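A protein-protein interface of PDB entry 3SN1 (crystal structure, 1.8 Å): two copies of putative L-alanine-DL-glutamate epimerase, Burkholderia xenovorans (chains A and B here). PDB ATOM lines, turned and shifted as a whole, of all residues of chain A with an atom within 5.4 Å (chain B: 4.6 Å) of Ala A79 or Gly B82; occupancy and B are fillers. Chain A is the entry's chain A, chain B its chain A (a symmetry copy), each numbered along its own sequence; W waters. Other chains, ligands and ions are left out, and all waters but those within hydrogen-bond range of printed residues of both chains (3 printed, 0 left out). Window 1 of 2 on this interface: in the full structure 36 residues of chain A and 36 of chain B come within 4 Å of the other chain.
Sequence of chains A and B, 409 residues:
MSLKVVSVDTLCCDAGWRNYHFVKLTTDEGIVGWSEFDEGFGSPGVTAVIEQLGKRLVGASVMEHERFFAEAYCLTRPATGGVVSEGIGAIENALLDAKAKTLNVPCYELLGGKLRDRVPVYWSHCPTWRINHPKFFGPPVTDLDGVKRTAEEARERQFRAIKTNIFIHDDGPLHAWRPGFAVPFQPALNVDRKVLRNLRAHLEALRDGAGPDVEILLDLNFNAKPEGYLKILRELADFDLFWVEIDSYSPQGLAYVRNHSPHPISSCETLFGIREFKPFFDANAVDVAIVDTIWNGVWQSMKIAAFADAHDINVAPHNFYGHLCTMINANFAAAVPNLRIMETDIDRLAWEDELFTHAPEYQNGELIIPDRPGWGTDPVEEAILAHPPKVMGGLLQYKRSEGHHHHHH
The backbone carbonyl oxygen of Pro A78 sits at hydrogen-bond distance from the side-chain hydroxyl of Tyr B249 (3.3 Å). The side-chain hydroxyl (OH) of Tyr B249 is in hydrogen-bond range of the backbone carbonyl oxygen (O) of Arg A77 (2.7 Å).
The side-chain carboxylate (OE2) of Glu B86 is in hydrogen-bond range of the side-chain hydroxyl (OG) of Ser B43 (2.6 Å). The side-chain carboxylate of Glu B86 sits at hydrogen-bond distance from the indole nitrogen of Trp B295 (3.3 Å).
Among the printed residues, merely in contact across the chains: Ala A79 with Ser B43 (3.3 Å), Pro A78 with Trp B295 (3.4 Å), Ala A79 with Gly B42 (3.5 Å), Thr A80 with Tyr B249 (3.5 Å), Ala A79 with Glu B86 (3.5 Å), Thr A76 with Gly B42 (3.6 Å), Val A84 with Val B83 (3.8 Å) and Ala A79 with Gly B82 (3.99 Å).
Of the printed residues of chain A, Gly B82 touches Ala A79. Printed residues of chain A within 4 Å of Tyr B249: Arg A77, Pro A78 and Thr A80. Printed residues of chain A within 4 Å of Glu B86: Ala A79. Printed residues of chain A within 4 Å of Gly B42: Thr A76 (3.6 Å) and Ala A79 (3.5 Å). Printed residues of chain A within 4 Å of Val B83: Val A84 (3.8 Å). Printed residues of chain B within 4 Å of Thr A80: Tyr B249. Thr B80 touches none of the printed residues of chain A. Gly A81 touches none of the printed residues of chain B. The nearest printed residue of chain A that does not touch Trp B295 is Ala A79 (4.2 Å).
Of the 7 printed residues of chain A, 6 touch a printed residue of chain B. Printed residues of chain A that touch a printed residue of chain B: Thr A76, Arg A77, Pro A78, Ala A79, Thr A80 and Val A84. Hydrophobic or aromatic side chains of chain A that line the printed part of chain B: Pro A78, Ala A79 and Val A84. Hydrophobic or aromatic side chains of chain B within 4 Å of the printed part of chain A: Val B83, Tyr B249 and Trp B295. Among the printed residues, no Asp or Glu carboxylate lies within 4 Å of a Lys or Arg side-chain nitrogen of the other chain.
3 positions are printed for both chains. Of the 10 pairs that touch across the chains among the printed residues, none has its exchanged pair printed and touching as well.
Water W1 lies within hydrogen-bond range of the side-chain hydroxyl (OH) of Tyr B249 and the backbone carbonyl oxygen (O) of Pro A78. Water W2 bridges the backbone carbonyl oxygen (O) of Thr A80 (2.8 Å) and the backbone NH (N) of Gly B82 (3.4 Å). Water W3 lies within hydrogen-bond range of O of Ala A79, O of Gly A81, N of Val B83 and N of Val A84.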
ATOM      1  N   THR A  76      11.551 -18.301 -15.792  1.00  0.00           N
ATOM      2  CA  THR A  76      12.062 -19.531 -15.189  1.00  0.00           C
ATOM      3  C   THR A  76      12.143 -20.693 -16.186  1.00  0.00           C
ATOM      4  O   THR A  76      12.287 -21.853 -15.781  1.00  0.00           O
ATOM      5  CB  THR A  76      11.184 -19.964 -14.002  1.00  0.00           C
ATOM      6  OG1 THR A  76       9.832 -20.218 -14.431  1.00  0.00           O
ATOM      7  CG2 THR A  76      11.183 -18.871 -12.887  1.00  0.00           C
ATOM      8  N   ARG A  77      12.079 -20.380 -17.478  1.00  0.00           N
ATOM      9  CA  ARG A  77      11.959 -21.405 -18.524  1.00  0.00           C
ATOM     10  C   ARG A  77      13.020 -22.511 -18.418  1.00  0.00           C
ATOM     11  O   ARG A  77      12.684 -23.685 -18.568  1.00  0.00           O
ATOM     12  CB  ARG A  77      12.017 -20.727 -19.890  1.00  0.00           C
ATOM     13  CG  ARG A  77      11.153 -21.322 -20.952  1.00  0.00           C
ATOM     14  CD  ARG A  77      11.356 -20.549 -22.280  1.00  0.00           C
ATOM     15  NE  ARG A  77      10.254 -20.879 -23.184  1.00  0.00           N
ATOM     16  CZ  ARG A  77       9.282 -20.056 -23.567  1.00  0.00           C
ATOM     17  NH1 ARG A  77       9.250 -18.762 -23.229  1.00  0.00           N
ATOM     18  NH2 ARG A  77       8.322 -20.560 -24.329  1.00  0.00           N
ATOM     19  N   PRO A  78      14.291 -22.144 -18.151  1.00  0.00           N
ATOM     20  CA  PRO A  78      15.334 -23.189 -18.110  1.00  0.00           C
ATOM     21  C   PRO A  78      15.156 -24.263 -17.036  1.00  0.00           C
ATOM     22  O   PRO A  78      15.633 -25.399 -17.221  1.00  0.00           O
ATOM     23  CB  PRO A  78      16.618 -22.399 -17.862  1.00  0.00           C
ATOM     24  CG  PRO A  78      16.321 -20.997 -18.392  1.00  0.00           C
ATOM     25  CD  PRO A  78      14.878 -20.794 -18.027  1.00  0.00           C
ATOM     26  N   ALA A  79      14.522 -23.901 -15.924  1.00  0.00           N
ATOM     27  CA  ALA A  79      14.352 -24.812 -14.781  1.00  0.00           C
ATOM     28  C   ALA A  79      12.878 -25.068 -14.487  1.00  0.00           C
ATOM     29  O   ALA A  79      12.477 -25.325 -13.347  1.00  0.00           O
ATOM     30  CB  ALA A  79      15.093 -24.220 -13.543  1.00  0.00           C
ATOM     31  N   THR A  80      12.068 -25.047 -15.540  1.00  0.00           N
ATOM     32  CA  THR A  80      10.643 -25.285 -15.420  1.00  0.00           C
ATOM     33  C   THR A  80      10.316 -26.712 -14.952  1.00  0.00           C
ATOM     34  O   THR A  80      11.137 -27.655 -15.068  1.00  0.00           O
ATOM     35  CB  THR A  80       9.886 -24.943 -16.741  1.00  0.00           C
ATOM     36  OG1 THR A  80       8.499 -24.751 -16.452  1.00  0.00           O
ATOM     37  CG2 THR A  80      10.053 -26.053 -17.806  1.00  0.00           C
ATOM     38  N   GLY A  81       9.113 -26.844 -14.421  1.00  0.00           N
ATOM     39  CA  GLY A  81       8.663 -28.071 -13.770  1.00  0.00           C
ATOM     40  C   GLY A  81       9.017 -28.047 -12.312  1.00  0.00           C
ATOM     41  O   GLY A  81       9.578 -27.086 -11.817  1.00  0.00           O
ATOM     42  N   VAL A  84       9.874 -24.972  -9.221  1.00  0.00           N
ATOM     43  CA  VAL A  84       9.564 -23.731  -9.952  1.00  0.00           C
ATOM     44  C   VAL A  84       8.088 -23.695 -10.360  1.00  0.00           C
ATOM     45  O   VAL A  84       7.373 -22.742 -10.087  1.00  0.00           O
ATOM     46  CB  VAL A  84      10.481 -23.561 -11.183  1.00  0.00           C
ATOM     47  CG1 VAL A  84       9.921 -22.509 -12.175  1.00  0.00           C
ATOM     48  CG2 VAL A  84      11.883 -23.186 -10.735  1.00  0.00           C
ATOM     49  N   GLY B  42      17.026 -18.733 -14.175  1.00  0.00           N
ATOM     50  CA  GLY B  42      15.664 -19.233 -13.988  1.00  0.00           C
ATOM     51  C   GLY B  42      15.444 -20.172 -12.813  1.00  0.00           C
ATOM     52  O   GLY B  42      14.466 -20.898 -12.806  1.00  0.00           O
ATOM     53  N   SER B  43      16.319 -20.105 -11.797  1.00  0.00           N
ATOM     54  CA  SER B  43      16.408 -21.167 -10.799  1.00  0.00           C
ATOM     55  C   SER B  43      16.407 -20.659  -9.341  1.00  0.00           C
ATOM     56  O   SER B  43      17.338 -20.955  -8.590  1.00  0.00           O
ATOM     57  CB  SER B  43      17.688 -21.976 -11.049  1.00  0.00           C
ATOM     58  OG  SER B  43      17.701 -22.589 -12.359  1.00  0.00           O
ATOM     59  N   THR B  80      11.311 -34.010  -8.869  1.00  0.00           N
ATOM     60  CA  THR B  80      12.617 -34.134  -9.488  1.00  0.00           C
ATOM     61  C   THR B  80      12.748 -33.296 -10.771  1.00  0.00           C
ATOM     62  O   THR B  80      11.743 -32.903 -11.414  1.00  0.00           O
ATOM     63  CB  THR B  80      12.992 -35.624  -9.755  1.00  0.00           C
ATOM     64  OG1 THR B  80      14.408 -35.730  -9.924  1.00  0.00           O
ATOM     65  CG2 THR B  80      12.268 -36.188 -11.002  1.00  0.00           C
ATOM     66  N   GLY B  81      13.995 -33.029 -11.116  1.00  0.00           N
ATOM     67  CA  GLY B  81      14.340 -32.118 -12.204  1.00  0.00           C
ATOM     68  C   GLY B  81      14.460 -30.715 -11.690  1.00  0.00           C
ATOM     69  O   GLY B  81      14.302 -30.462 -10.508  1.00  0.00           O
ATOM     70  N   GLY B  82      14.761 -29.788 -12.588  1.00  0.00           N
ATOM     71  CA  GLY B  82      14.788 -28.378 -12.238  1.00  0.00           C
ATOM     72  C   GLY B  82      15.598 -28.068 -10.994  1.00  0.00           C
ATOM     73  O   GLY B  82      16.717 -28.590 -10.791  1.00  0.00           O
ATOM     74  N   VAL B  83      15.037 -27.220 -10.156  1.00  0.00           N
ATOM     75  CA  VAL B  83      15.766 -26.664  -9.017  1.00  0.00           C
ATOM     76  C   VAL B  83      16.152 -27.750  -8.003  1.00  0.00           C
ATOM     77  O   VAL B  83      17.238 -27.694  -7.436  1.00  0.00           O
ATOM     78  CB  VAL B  83      14.954 -25.514  -8.389  1.00  0.00           C
ATOM     79  CG1 VAL B  83      15.322 -25.287  -6.935  1.00  0.00           C
ATOM     80  CG2 VAL B  83      15.184 -24.244  -9.213  1.00  0.00           C
ATOM     81  N   VAL B  84      15.283 -28.734  -7.797  1.00  0.00           N
ATOM     82  CA  VAL B  84      15.620 -29.889  -6.949  1.00  0.00           C
ATOM     83  C   VAL B  84      16.872 -30.600  -7.473  1.00  0.00           C
ATOM     84  O   VAL B  84      17.828 -30.829  -6.745  1.00  0.00           O
ATOM     85  CB  VAL B  84      14.434 -30.873  -6.840  1.00  0.00           C
ATOM     86  CG1 VAL B  84      14.883 -32.259  -6.309  1.00  0.00           C
ATOM     87  CG2 VAL B  84      13.353 -30.280  -5.953  1.00  0.00           C
ATOM     88  N   SER B  85      16.882 -30.911  -8.763  1.00  0.00           N
ATOM     89  CA  SER B  85      18.011 -31.633  -9.340  1.00  0.00           C
ATOM     90  C   SER B  85      19.273 -30.784  -9.361  1.00  0.00           C
ATOM     91  O   SER B  85      20.378 -31.314  -9.178  1.00  0.00           O
ATOM     92  CB  SER B  85      17.653 -32.169 -10.728  1.00  0.00           C
ATOM     93  OG  SER B  85      16.799 -33.283 -10.593  1.00  0.00           O
ATOM     94  N   GLU B  86      19.123 -29.465  -9.520  1.00  0.00           N
ATOM     95  CA  GLU B  86      20.267 -28.560  -9.390  1.00  0.00           C
ATOM     96  C   GLU B  86      20.906 -28.610  -7.999  1.00  0.00           C
ATOM     97  O   GLU B  86      22.139 -28.573  -7.867  1.00  0.00           O
ATOM     98  CB  GLU B  86      19.868 -27.118  -9.710  1.00  0.00           C
ATOM     99  CG  GLU B  86      19.599 -26.843 -11.189  1.00  0.00           C
ATOM    100  CD  GLU B  86      19.239 -25.410 -11.441  1.00  0.00           C
ATOM    101  OE1 GLU B  86      20.009 -24.529 -11.015  1.00  0.00           O
ATOM    102  OE2 GLU B  86      18.139 -25.156 -12.007  1.00  0.00           O
ATOM    103  N   TYR B 249      11.478 -27.841 -25.498  1.00  0.00           N
ATOM    104  CA  TYR B 249      10.889 -28.926 -24.741  1.00  0.00           C
ATOM    105  C   TYR B 249      10.012 -29.815 -25.628  1.00  0.00           C
ATOM    106  O   TYR B 249       9.229 -30.641 -25.122  1.00  0.00           O
ATOM    107  CB  TYR B 249      10.135 -28.401 -23.540  1.00  0.00           C
ATOM    108  CG  TYR B 249      11.041 -27.732 -22.506  1.00  0.00           C
ATOM    109  CD1 TYR B 249      12.256 -28.314 -22.131  1.00  0.00           C
ATOM    110  CD2 TYR B 249      10.700 -26.507 -21.928  1.00  0.00           C
ATOM    111  CE1 TYR B 249      13.079 -27.710 -21.198  1.00  0.00           C
ATOM    112  CE2 TYR B 249      11.538 -25.899 -20.973  1.00  0.00           C
ATOM    113  CZ  TYR B 249      12.722 -26.506 -20.624  1.00  0.00           C
ATOM    114  OH  TYR B 249      13.566 -25.941 -19.697  1.00  0.00           O
ATOM    115  N   PHE B 272      17.944 -32.693 -17.658  1.00  0.00           N
ATOM    116  CA  PHE B 272      18.466 -33.458 -16.533  1.00  0.00           C
ATOM    117  C   PHE B 272      18.355 -34.967 -16.741  1.00  0.00           C
ATOM    118  O   PHE B 272      17.268 -35.494 -16.888  1.00  0.00           O
ATOM    119  CB  PHE B 272      17.704 -33.114 -15.251  1.00  0.00           C
ATOM    120  CG  PHE B 272      17.838 -31.688 -14.790  1.00  0.00           C
ATOM    121  CD1 PHE B 272      18.769 -31.349 -13.836  1.00  0.00           C
ATOM    122  CD2 PHE B 272      17.009 -30.691 -15.299  1.00  0.00           C
ATOM    123  CE1 PHE B 272      18.876 -30.040 -13.396  1.00  0.00           C
ATOM    124  CE2 PHE B 272      17.120 -29.380 -14.863  1.00  0.00           C
ATOM    125  CZ  PHE B 272      18.045 -29.068 -13.904  1.00  0.00           C
ATOM    126  N   TRP B 295      24.531 -28.243 -13.144  1.00  0.00           N
ATOM    127  CA  TRP B 295      23.173 -28.636 -12.826  1.00  0.00           C
ATOM    128  C   TRP B 295      23.028 -30.126 -12.485  1.00  0.00           C
ATOM    129  O   TRP B 295      22.377 -30.488 -11.519  1.00  0.00           O
ATOM    130  CB  TRP B 295      22.278 -28.319 -14.045  1.00  0.00           C
ATOM    131  CG  TRP B 295      21.860 -26.898 -14.119  1.00  0.00           C
ATOM    132  CD1 TRP B 295      22.442 -25.822 -13.505  1.00  0.00           C
ATOM    133  CD2 TRP B 295      20.686 -26.404 -14.773  1.00  0.00           C
ATOM    134  NE1 TRP B 295      21.721 -24.673 -13.786  1.00  0.00           N
ATOM    135  CE2 TRP B 295      20.636 -25.018 -14.556  1.00  0.00           C
ATOM    136  CE3 TRP B 295      19.689 -27.007 -15.559  1.00  0.00           C
ATOM    137  CZ2 TRP B 295      19.600 -24.222 -15.057  1.00  0.00           C
ATOM    138  CZ3 TRP B 295      18.671 -26.206 -16.060  1.00  0.00           C
ATOM    139  CH2 TRP B 295      18.641 -24.837 -15.803  1.00  0.00           C
HETATM  140  O   HOH W   1      14.753 -27.920 -18.168  1.00  0.00           O
HETATM  141  O   HOH W   2      13.812 -28.299 -15.463  1.00  0.00           O
HETATM  142  O   HOH W   3      12.237 -26.456 -10.814  1.00  0.00           O
